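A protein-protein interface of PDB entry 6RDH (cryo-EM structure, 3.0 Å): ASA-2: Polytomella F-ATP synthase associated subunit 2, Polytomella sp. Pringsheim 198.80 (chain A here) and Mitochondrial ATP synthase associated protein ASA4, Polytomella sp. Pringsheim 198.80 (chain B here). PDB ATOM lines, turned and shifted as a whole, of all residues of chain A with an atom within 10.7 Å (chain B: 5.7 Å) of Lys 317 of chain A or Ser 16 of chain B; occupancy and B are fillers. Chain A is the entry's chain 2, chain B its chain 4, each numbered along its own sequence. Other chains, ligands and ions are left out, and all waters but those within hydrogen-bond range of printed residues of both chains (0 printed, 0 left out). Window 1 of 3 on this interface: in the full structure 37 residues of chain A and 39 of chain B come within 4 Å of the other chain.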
ATOM      1  N   GLU A 277      -5.675 -11.852 -14.638  1.00  0.00           N
ATOM      2  CA  GLU A 277      -6.587 -11.744 -13.513  1.00  0.00           C
ATOM      3  C   GLU A 277      -5.978 -12.394 -12.279  1.00  0.00           C
ATOM      4  O   GLU A 277      -5.048 -13.195 -12.370  1.00  0.00           O
ATOM      5  CB  GLU A 277      -7.945 -12.372 -13.843  1.00  0.00           C
ATOM      6  CG  GLU A 277      -7.992 -13.896 -13.922  1.00  0.00           C
ATOM      7  CD  GLU A 277      -7.293 -14.478 -15.143  1.00  0.00           C
ATOM      8  OE1 GLU A 277      -6.972 -15.684 -15.128  1.00  0.00           O
ATOM      9  OE2 GLU A 277      -7.064 -13.732 -16.118  1.00  0.00           O
ATOM     10  N   VAL A 278      -6.513 -12.031 -11.109  1.00  0.00           N
ATOM     11  CA  VAL A 278      -5.873 -12.413  -9.855  1.00  0.00           C
ATOM     12  C   VAL A 278      -6.036 -13.887  -9.522  1.00  0.00           C
ATOM     13  O   VAL A 278      -5.342 -14.381  -8.629  1.00  0.00           O
ATOM     14  CB  VAL A 278      -6.397 -11.571  -8.686  1.00  0.00           C
ATOM     15  CG1 VAL A 278      -6.200 -10.100  -8.964  1.00  0.00           C
ATOM     16  CG2 VAL A 278      -7.834 -11.887  -8.463  1.00  0.00           C
ATOM     17  N   SER A 279      -6.926 -14.614 -10.194  1.00  0.00           N
ATOM     18  CA  SER A 279      -6.916 -16.058 -10.013  1.00  0.00           C
ATOM     19  C   SER A 279      -5.665 -16.660 -10.629  1.00  0.00           C
ATOM     20  O   SER A 279      -5.026 -17.527 -10.028  1.00  0.00           O
ATOM     21  CB  SER A 279      -8.175 -16.686 -10.606  1.00  0.00           C
ATOM     22  OG  SER A 279      -8.166 -16.610 -12.015  1.00  0.00           O
ATOM     23  N   SER A 280      -5.265 -16.163 -11.800  1.00  0.00           N
ATOM     24  CA  SER A 280      -4.010 -16.603 -12.394  1.00  0.00           C
ATOM     25  C   SER A 280      -2.809 -16.096 -11.612  1.00  0.00           C
ATOM     26  O   SER A 280      -1.804 -16.795 -11.517  1.00  0.00           O
ATOM     27  CB  SER A 280      -3.912 -16.149 -13.845  1.00  0.00           C
ATOM     28  OG  SER A 280      -4.875 -16.797 -14.654  1.00  0.00           O
ATOM     29  N   LEU A 309      -4.758 -11.268  -1.877  1.00  0.00           N
ATOM     30  CA  LEU A 309      -5.961 -10.648  -2.428  1.00  0.00           C
ATOM     31  C   LEU A 309      -6.984 -11.692  -2.847  1.00  0.00           C
ATOM     32  O   LEU A 309      -8.157 -11.607  -2.474  1.00  0.00           O
ATOM     33  CB  LEU A 309      -5.605  -9.770  -3.620  1.00  0.00           C
ATOM     34  CG  LEU A 309      -5.117  -8.359  -3.349  1.00  0.00           C
ATOM     35  CD1 LEU A 309      -4.838  -7.691  -4.660  1.00  0.00           C
ATOM     36  CD2 LEU A 309      -6.157  -7.595  -2.589  1.00  0.00           C
ATOM     37  N   ALA A 310      -6.557 -12.697  -3.612  1.00  0.00           N
ATOM     38  CA  ALA A 310      -7.496 -13.720  -4.047  1.00  0.00           C
ATOM     39  C   ALA A 310      -7.973 -14.581  -2.888  1.00  0.00           C
ATOM     40  O   ALA A 310      -9.127 -15.021  -2.886  1.00  0.00           O
ATOM     41  CB  ALA A 310      -6.863 -14.585  -5.126  1.00  0.00           C
ATOM     42  N   ALA A 311      -7.135 -14.764  -1.864  1.00  0.00           N
ATOM     43  CA  ALA A 311      -7.519 -15.581  -0.720  1.00  0.00           C
ATOM     44  C   ALA A 311      -8.584 -14.898   0.123  1.00  0.00           C
ATOM     45  O   ALA A 311      -9.614 -15.506   0.439  1.00  0.00           O
ATOM     46  CB  ALA A 311      -6.289 -15.904   0.124  1.00  0.00           C
ATOM     47  N   ASP A 312      -8.380 -13.628   0.489  1.00  0.00           N
ATOM     48  CA  ASP A 312      -9.431 -13.017   1.295  1.00  0.00           C
ATOM     49  C   ASP A 312     -10.627 -12.573   0.458  1.00  0.00           C
ATOM     50  O   ASP A 312     -11.709 -12.373   1.018  1.00  0.00           O
ATOM     51  CB  ASP A 312      -8.898 -11.866   2.167  1.00  0.00           C
ATOM     52  CG  ASP A 312      -8.150 -10.797   1.397  1.00  0.00           C
ATOM     53  OD1 ASP A 312      -8.310 -10.674   0.175  1.00  0.00           O
ATOM     54  OD2 ASP A 312      -7.386 -10.046   2.038  1.00  0.00           O
ATOM     55  N   ALA A 313     -10.486 -12.467  -0.866  1.00  0.00           N
ATOM     56  CA  ALA A 313     -11.667 -12.259  -1.690  1.00  0.00           C
ATOM     57  C   ALA A 313     -12.498 -13.527  -1.792  1.00  0.00           C
ATOM     58  O   ALA A 313     -13.726 -13.457  -1.868  1.00  0.00           O
ATOM     59  CB  ALA A 313     -11.266 -11.776  -3.076  1.00  0.00           C
ATOM     60  N   ALA A 314     -11.856 -14.696  -1.805  1.00  0.00           N
ATOM     61  CA  ALA A 314     -12.628 -15.932  -1.768  1.00  0.00           C
ATOM     62  C   ALA A 314     -13.179 -16.201  -0.379  1.00  0.00           C
ATOM     63  O   ALA A 314     -14.165 -16.929  -0.237  1.00  0.00           O
ATOM     64  CB  ALA A 314     -11.777 -17.107  -2.231  1.00  0.00           C
ATOM     65  N   ARG A 315     -12.538 -15.651   0.652  1.00  0.00           N
ATOM     66  CA  ARG A 315     -13.109 -15.704   1.995  1.00  0.00           C
ATOM     67  C   ARG A 315     -14.341 -14.816   2.103  1.00  0.00           C
ATOM     68  O   ARG A 315     -15.321 -15.182   2.760  1.00  0.00           O
ATOM     69  CB  ARG A 315     -12.061 -15.284   3.022  1.00  0.00           C
ATOM     70  CG  ARG A 315     -12.571 -15.218   4.440  1.00  0.00           C
ATOM     71  CD  ARG A 315     -11.510 -14.758   5.390  1.00  0.00           C
ATOM     72  NE  ARG A 315     -11.916 -14.935   6.777  1.00  0.00           N
ATOM     73  CZ  ARG A 315     -12.486 -13.994   7.517  1.00  0.00           C
ATOM     74  NH1 ARG A 315     -12.716 -12.795   7.008  1.00  0.00           N
ATOM     75  NH2 ARG A 315     -12.818 -14.252   8.771  1.00  0.00           N
ATOM     76  N   LEU A 316     -14.305 -13.648   1.457  1.00  0.00           N
ATOM     77  CA  LEU A 316     -15.405 -12.693   1.539  1.00  0.00           C
ATOM     78  C   LEU A 316     -16.664 -13.210   0.862  1.00  0.00           C
ATOM     79  O   LEU A 316     -17.773 -12.940   1.331  1.00  0.00           O
ATOM     80  CB  LEU A 316     -14.988 -11.378   0.898  1.00  0.00           C
ATOM     81  CG  LEU A 316     -15.526 -10.103   1.515  1.00  0.00           C
ATOM     82  CD1 LEU A 316     -15.183 -10.084   2.979  1.00  0.00           C
ATOM     83  CD2 LEU A 316     -14.930  -8.912   0.815  1.00  0.00           C
ATOM     84  N   LYS A 317     -16.516 -13.961  -0.224  1.00  0.00           N
ATOM     85  CA  LYS A 317     -17.641 -14.537  -0.953  1.00  0.00           C
ATOM     86  C   LYS A 317     -17.854 -15.995  -0.589  1.00  0.00           C
ATOM     87  O   LYS A 317     -18.144 -16.814  -1.462  1.00  0.00           O
ATOM     88  CB  LYS A 317     -17.429 -14.396  -2.454  1.00  0.00           C
ATOM     89  CG  LYS A 317     -17.177 -12.988  -2.930  1.00  0.00           C
ATOM     90  CD  LYS A 317     -17.336 -12.913  -4.433  1.00  0.00           C
ATOM     91  CE  LYS A 317     -16.854 -11.588  -4.966  1.00  0.00           C
ATOM     92  NZ  LYS A 317     -17.283 -11.340  -6.368  1.00  0.00           N
ATOM     93  N   ARG A 318     -17.677 -16.343   0.683  1.00  0.00           N
ATOM     94  CA  ARG A 318     -17.743 -17.726   1.132  1.00  0.00           C
ATOM     95  C   ARG A 318     -19.158 -18.278   1.021  1.00  0.00           C
ATOM     96  O   ARG A 318     -20.143 -17.579   1.264  1.00  0.00           O
ATOM     97  CB  ARG A 318     -17.264 -17.827   2.575  1.00  0.00           C
ATOM     98  CG  ARG A 318     -16.939 -19.221   3.039  1.00  0.00           C
ATOM     99  CD  ARG A 318     -16.291 -19.179   4.389  1.00  0.00           C
ATOM    100  NE  ARG A 318     -14.848 -19.087   4.266  1.00  0.00           N
ATOM    101  CZ  ARG A 318     -14.060 -18.587   5.204  1.00  0.00           C
ATOM    102  NH1 ARG A 318     -14.585 -18.134   6.332  1.00  0.00           N
ATOM    103  NH2 ARG A 318     -12.751 -18.544   5.022  1.00  0.00           N
ATOM    104  N   SER A 319     -19.248 -19.558   0.671  1.00  0.00           N
ATOM    105  CA  SER A 319     -20.475 -20.257   0.307  1.00  0.00           C
ATOM    106  C   SER A 319     -21.446 -20.442   1.435  1.00  0.00           C
ATOM    107  O   SER A 319     -22.360 -21.209   1.156  1.00  0.00           O
ATOM    108  CB  SER A 319     -20.142 -21.626  -0.285  1.00  0.00           C
ATOM    109  OG  SER A 319     -19.645 -22.509   0.699  1.00  0.00           O
ATOM    110  N   SER A 320     -21.268 -19.940   2.660  1.00  0.00           N
ATOM    111  CA  SER A 320     -22.267 -19.907   3.735  1.00  0.00           C
ATOM    112  C   SER A 320     -22.694 -21.270   4.279  1.00  0.00           C
ATOM    113  O   SER A 320     -23.521 -21.343   5.190  1.00  0.00           O
ATOM    114  CB  SER A 320     -23.513 -19.141   3.304  1.00  0.00           C
ATOM    115  OG  SER A 320     -24.593 -19.480   4.153  1.00  0.00           O
ATOM    116  N   ALA A 321     -22.163 -22.349   3.720  1.00  0.00           N
ATOM    117  CA  ALA A 321     -22.092 -23.632   4.390  1.00  0.00           C
ATOM    118  C   ALA A 321     -20.659 -24.015   4.681  1.00  0.00           C
ATOM    119  O   ALA A 321     -20.419 -24.846   5.557  1.00  0.00           O
ATOM    120  CB  ALA A 321     -22.748 -24.729   3.540  1.00  0.00           C
ATOM    121  N   GLU A 322     -19.716 -23.435   3.942  1.00  0.00           N
ATOM    122  CA  GLU A 322     -18.333 -23.384   4.376  1.00  0.00           C
ATOM    123  C   GLU A 322     -18.174 -22.475   5.585  1.00  0.00           C
ATOM    124  O   GLU A 322     -17.321 -22.728   6.440  1.00  0.00           O
ATOM    125  CB  GLU A 322     -17.457 -22.908   3.222  1.00  0.00           C
ATOM    126  CG  GLU A 322     -15.972 -22.850   3.506  1.00  0.00           C
ATOM    127  CD  GLU A 322     -15.193 -22.307   2.334  1.00  0.00           C
ATOM    128  OE1 GLU A 322     -15.741 -22.296   1.214  1.00  0.00           O
ATOM    129  OE2 GLU A 322     -14.034 -21.891   2.534  1.00  0.00           O
ATOM    130  N   SER A 323     -18.997 -21.434   5.698  1.00  0.00           N
ATOM    131  CA  SER A 323     -18.826 -20.497   6.802  1.00  0.00           C
ATOM    132  C   SER A 323     -19.314 -21.088   8.118  1.00  0.00           C
ATOM    133  O   SER A 323     -18.645 -20.951   9.152  1.00  0.00           O
ATOM    134  CB  SER A 323     -19.550 -19.193   6.492  1.00  0.00           C
ATOM    135  OG  SER A 323     -19.349 -18.258   7.531  1.00  0.00           O
ATOM    136  N   VAL A 361      -6.501 -12.669   5.959  1.00  0.00           N
ATOM    137  CA  VAL A 361      -6.945 -13.001   7.304  1.00  0.00           C
ATOM    138  C   VAL A 361      -7.281 -14.488   7.356  1.00  0.00           C
ATOM    139  O   VAL A 361      -7.912 -15.034   6.444  1.00  0.00           O
ATOM    140  CB  VAL A 361      -8.115 -12.089   7.760  1.00  0.00           C
ATOM    141  CG1 VAL A 361      -9.329 -12.196   6.862  1.00  0.00           C
ATOM    142  CG2 VAL A 361      -8.490 -12.349   9.209  1.00  0.00           C
ATOM    143  N   ASP A 363      -8.738 -17.926   9.429  1.00  0.00           N
ATOM    144  CA  ASP A 363      -9.911 -18.124  10.268  1.00  0.00           C
ATOM    145  C   ASP A 363      -9.567 -18.762  11.603  1.00  0.00           C
ATOM    146  O   ASP A 363     -10.081 -18.344  12.643  1.00  0.00           O
ATOM    147  CB  ASP A 363     -10.942 -18.963   9.532  1.00  0.00           C
ATOM    148  CG  ASP A 363     -11.878 -18.121   8.717  1.00  0.00           C
ATOM    149  OD1 ASP A 363     -12.002 -16.910   8.999  1.00  0.00           O
ATOM    150  OD2 ASP A 363     -12.490 -18.671   7.791  1.00  0.00           O
ATOM    151  N   PRO A 379     -14.983 -27.932   2.640  1.00  0.00           N
ATOM    152  CA  PRO A 379     -16.391 -28.325   2.830  1.00  0.00           C
ATOM    153  C   PRO A 379     -16.973 -29.408   1.927  1.00  0.00           C
ATOM    154  O   PRO A 379     -17.080 -30.562   2.347  1.00  0.00           O
ATOM    155  CB  PRO A 379     -17.136 -27.003   2.613  1.00  0.00           C
ATOM    156  CG  PRO A 379     -16.204 -26.153   1.818  1.00  0.00           C
ATOM    157  CD  PRO A 379     -14.831 -26.536   2.199  1.00  0.00           C
ATOM    158  N   SER A 381     -17.139 -28.258  -1.770  1.00  0.00           N
ATOM    159  CA  SER A 381     -16.797 -27.637  -3.040  1.00  0.00           C
ATOM    160  C   SER A 381     -15.360 -27.925  -3.420  1.00  0.00           C
ATOM    161  O   SER A 381     -14.996 -27.824  -4.595  1.00  0.00           O
ATOM    162  CB  SER A 381     -17.035 -26.131  -2.968  1.00  0.00           C
ATOM    163  OG  SER A 381     -16.136 -25.514  -2.072  1.00  0.00           O
ATOM    164  N   LEU A 382     -14.531 -28.270  -2.441  1.00  0.00           N
ATOM    165  CA  LEU A 382     -13.156 -28.674  -2.674  1.00  0.00           C
ATOM    166  C   LEU A 382     -12.949 -30.138  -2.310  1.00  0.00           C
ATOM    167  O   LEU A 382     -11.872 -30.532  -1.872  1.00  0.00           O
ATOM    168  CB  LEU A 382     -12.199 -27.776  -1.900  1.00  0.00           C
ATOM    169  CG  LEU A 382     -12.232 -26.318  -2.328  1.00  0.00           C
ATOM    170  CD1 LEU A 382     -11.927 -25.413  -1.164  1.00  0.00           C
ATOM    171  CD2 LEU A 382     -11.224 -26.116  -3.433  1.00  0.00           C
ATOM    172  N   LEU B  12     -12.193  -6.416  -3.272  1.00  0.00           N
ATOM    173  CA  LEU B  12     -12.250  -7.867  -3.173  1.00  0.00           C
ATOM    174  C   LEU B  12     -13.515  -8.416  -3.802  1.00  0.00           C
ATOM    175  O   LEU B  12     -13.514  -9.541  -4.307  1.00  0.00           O
ATOM    176  CB  LEU B  12     -12.178  -8.307  -1.715  1.00  0.00           C
ATOM    177  CG  LEU B  12     -10.989  -7.792  -0.922  1.00  0.00           C
ATOM    178  CD1 LEU B  12     -11.044  -8.312   0.491  1.00  0.00           C
ATOM    179  CD2 LEU B  12      -9.709  -8.198  -1.588  1.00  0.00           C
ATOM    180  N   TYR B  13     -14.601  -7.646  -3.771  1.00  0.00           N
ATOM    181  CA  TYR B  13     -15.806  -8.057  -4.476  1.00  0.00           C
ATOM    182  C   TYR B  13     -15.669  -7.887  -5.976  1.00  0.00           C
ATOM    183  O   TYR B  13     -16.269  -8.650  -6.740  1.00  0.00           O
ATOM    184  CB  TYR B  13     -17.012  -7.283  -3.962  1.00  0.00           C
ATOM    185  CG  TYR B  13     -17.788  -8.053  -2.938  1.00  0.00           C
ATOM    186  CD1 TYR B  13     -18.724  -8.986  -3.332  1.00  0.00           C
ATOM    187  CD2 TYR B  13     -17.571  -7.872  -1.589  1.00  0.00           C
ATOM    188  CE1 TYR B  13     -19.429  -9.708  -2.420  1.00  0.00           C
ATOM    189  CE2 TYR B  13     -18.281  -8.595  -0.662  1.00  0.00           C
ATOM    190  CZ  TYR B  13     -19.210  -9.511  -1.090  1.00  0.00           C
ATOM    191  OH  TYR B  13     -19.934 -10.247  -0.191  1.00  0.00           O
ATOM    192  N   PHE B  14     -14.876  -6.923  -6.419  1.00  0.00           N
ATOM    193  CA  PHE B  14     -14.797  -6.604  -7.834  1.00  0.00           C
ATOM    194  C   PHE B  14     -13.768  -7.446  -8.571  1.00  0.00           C
ATOM    195  O   PHE B  14     -13.600  -7.264  -9.778  1.00  0.00           O
ATOM    196  CB  PHE B  14     -14.463  -5.123  -8.042  1.00  0.00           C
ATOM    197  CG  PHE B  14     -15.421  -4.163  -7.391  1.00  0.00           C
ATOM    198  CD1 PHE B  14     -16.746  -4.494  -7.159  1.00  0.00           C
ATOM    199  CD2 PHE B  14     -14.989  -2.899  -7.041  1.00  0.00           C
ATOM    200  CE1 PHE B  14     -17.603  -3.599  -6.560  1.00  0.00           C
ATOM    201  CE2 PHE B  14     -15.845  -2.000  -6.448  1.00  0.00           C
ATOM    202  CZ  PHE B  14     -17.154  -2.352  -6.210  1.00  0.00           C
ATOM    203  N   LEU B  15     -13.069  -8.350  -7.881  1.00  0.00           N
ATOM    204  CA  LEU B  15     -12.098  -9.212  -8.549  1.00  0.00           C
ATOM    205  C   LEU B  15     -12.794 -10.229  -9.438  1.00  0.00           C
ATOM    206  O   LEU B  15     -12.382 -10.456 -10.580  1.00  0.00           O
ATOM    207  CB  LEU B  15     -11.222  -9.925  -7.519  1.00  0.00           C
ATOM    208  CG  LEU B  15     -10.211  -9.110  -6.714  1.00  0.00           C
ATOM    209  CD1 LEU B  15      -9.420  -9.981  -5.776  1.00  0.00           C
ATOM    210  CD2 LEU B  15      -9.283  -8.317  -7.608  1.00  0.00           C
ATOM    211  N   SER B  16     -13.850 -10.855  -8.929  1.00  0.00           N
ATOM    212  CA  SER B  16     -14.548 -11.889  -9.676  1.00  0.00           C
ATOM    213  C   SER B  16     -15.574 -11.341 -10.655  1.00  0.00           C
ATOM    214  O   SER B  16     -16.208 -12.132 -11.360  1.00  0.00           O
ATOM    215  CB  SER B  16     -15.244 -12.856  -8.719  1.00  0.00           C
ATOM    216  OG  SER B  16     -16.055 -13.768  -9.436  1.00  0.00           O
ATOM    217  N   SER B  17     -15.765 -10.028 -10.712  1.00  0.00           N
ATOM    218  CA  SER B  17     -16.706  -9.452 -11.656  1.00  0.00           C
ATOM    219  C   SER B  17     -16.008  -9.105 -12.963  1.00  0.00           C
ATOM    220  O   SER B  17     -14.804  -8.843 -13.007  1.00  0.00           O
ATOM    221  CB  SER B  17     -17.362  -8.201 -11.081  1.00  0.00           C
ATOM    222  OG  SER B  17     -16.424  -7.150 -10.995  1.00  0.00           O
ATOM    223  N   LYS B  18     -16.791  -9.099 -14.041  1.00  0.00           N
ATOM    224  CA  LYS B  18     -16.298  -8.746 -15.365  1.00  0.00           C
ATOM    225  C   LYS B  18     -16.912  -7.447 -15.869  1.00  0.00           C
ATOM    226  O   LYS B  18     -16.925  -7.198 -17.077  1.00  0.00           O
ATOM    227  CB  LYS B  18     -16.563  -9.877 -16.358  1.00  0.00           C
ATOM    228  CG  LYS B  18     -15.352 -10.749 -16.643  1.00  0.00           C
ATOM    229  CD  LYS B  18     -15.082 -11.699 -15.499  1.00  0.00           C
ATOM    230  CE  LYS B  18     -16.209 -12.694 -15.340  1.00  0.00           C
ATOM    231  NZ  LYS B  18     -15.878 -13.743 -14.337  1.00  0.00           N
ATOM    232  N   VAL B  62     -22.187  -4.758  -7.260  1.00  0.00           N
ATOM    233  CA  VAL B  62     -21.757  -5.650  -8.322  1.00  0.00           C
ATOM    234  C   VAL B  62     -23.008  -6.042  -9.092  1.00  0.00           C
ATOM    235  O   VAL B  62     -22.970  -6.233 -10.310  1.00  0.00           O
ATOM    236  CB  VAL B  62     -21.019  -6.874  -7.749  1.00  0.00           C
ATOM    237  CG1 VAL B  62     -20.581  -7.817  -8.838  1.00  0.00           C
ATOM    238  CG2 VAL B  62     -19.832  -6.439  -6.951  1.00  0.00           C
ATOM    239  N   ALA B  94     -23.568 -15.048  -9.135  1.00  0.00           N
ATOM    240  CA  ALA B  94     -22.321 -15.711  -8.773  1.00  0.00           C
ATOM    241  C   ALA B  94     -21.162 -14.727  -8.690  1.00  0.00           C
ATOM    242  O   ALA B  94     -20.298 -14.861  -7.822  1.00  0.00           O
ATOM    243  CB  ALA B  94     -22.006 -16.813  -9.773  1.00  0.00           C
ATOM    244  N   GLN B  95     -21.128 -13.731  -9.577  1.00  0.00           N
ATOM    245  CA  GLN B  95     -20.082 -12.716  -9.522  1.00  0.00           C
ATOM    246  C   GLN B  95     -20.237 -11.813  -8.315  1.00  0.00           C
ATOM    247  O   GLN B  95     -19.247 -11.266  -7.825  1.00  0.00           O
ATOM    248  CB  GLN B  95     -20.095 -11.853 -10.778  1.00  0.00           C
ATOM    249  CG  GLN B  95     -19.520 -12.492 -12.010  1.00  0.00           C
ATOM    250  CD  GLN B  95     -19.850 -11.704 -13.254  1.00  0.00           C
ATOM    251  OE1 GLN B  95     -20.113 -10.505 -13.190  1.00  0.00           O
ATOM    252  NE2 GLN B  95     -19.849 -12.376 -14.397  1.00  0.00           N
ATOM    253  N   ALA B  96     -21.459 -11.622  -7.845  1.00  0.00           N
ATOM    254  CA  ALA B  96     -21.699 -10.734  -6.722  1.00  0.00           C
ATOM    255  C   ALA B  96     -21.560 -11.412  -5.374  1.00  0.00           C
ATOM    256  O   ALA B  96     -21.713 -10.747  -4.350  1.00  0.00           O
ATOM    257  CB  ALA B  96     -23.085 -10.125  -6.824  1.00  0.00           C
ATOM    258  N   GLY B  97     -21.286 -12.703  -5.339  1.00  0.00           N
ATOM    259  CA  GLY B  97     -21.141 -13.400  -4.089  1.00  0.00           C
ATOM    260  C   GLY B  97     -22.393 -14.059  -3.576  1.00  0.00           C
ATOM    261  O   GLY B  97     -22.454 -14.381  -2.388  1.00  0.00           O
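The backbone carbonyl oxygen (O) of Tyr 13 of chain B lies within hydrogen-bond range of the side-chain amino group (NZ) of Lys 317 of chain A (2.9 Å). The backbone carbonyl oxygen of Gln 95 of chain B lies within hydrogen-bond range of the side-chain amino group of Lys 317 of chain A (2.4 Å).
The backbone carbonyl oxygen of Ser 16 of chain B is in hydrogen-bond range of the side-chain amino group of Lys 18 of chain B (3.4 Å).
Among the printed residues, pairs that only touch across the chains: Val 278 of chain A with Leu 15 of chain B, Leu 309 of chain A with Leu 12 of chain B, Leu 309 of chain A with Leu 15 of chain B, Asp 312 of chain A with Leu 12 of chain B, Ala 313 of chain A with Leu 12 of chain B, Ala 313 of chain A with Leu 15 of chain B, Leu 316 of chain A with Leu 12 of chain B, Leu 316 of chain A with Tyr 13 of chain B, Lys 317 of chain A with Leu 12 of chain B, Lys 317 of chain A with Ser 16 of chain B and Lys 317 of chain A with Gly 97 of chain B.
Lys 317 of chain A touches five residues of chain B. Printed residues of chain A within 4 Å of Tyr 13 of chain B: Leu 316 (3.7 Å) and Lys 317 (2.9 Å). No residue of chain A comes within 4 Å of Ser 17 of chain B. Of the printed residues of chain A, Gln 95 of chain B touches Lys 317 (2.4 Å). Gly 97 of chain B touches one residue of chain A. Of the printed residues of chain B, Ala 313 of chain A touches Leu 12 and Leu 15. Printed residues of chain B within 4 Å of Asp 312 of chain A: Leu 12 (3.3 Å). Of the printed residues of chain A, Leu 12 of chain B touches Leu 309 (3.7 Å), Asp 312 (3.3 Å), Ala 313 (3.4 Å), Leu 316 (3.8 Å) and Lys 317 (3.97 Å). Glu 277 of chain A touches none of the printed residues of chain B. The nearest printed residue of chain B that does not touch Val 278 of chain A is Ser 16 of chain B (6.1 Å).
Of the 12 printed residues of chain B, 6 touch a printed residue of chain A. Hydrophobic or aromatic side chains of chain B that line the printed part of chain A: Leu 12, Tyr 13 and Leu 15. Printed residues of chain A that touch a printed residue of chain B: Val 278, Leu 309, Asp 312, Ala 313, Leu 316 and Lys 317. Among the printed residues, 13 pairs touch across the chains.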
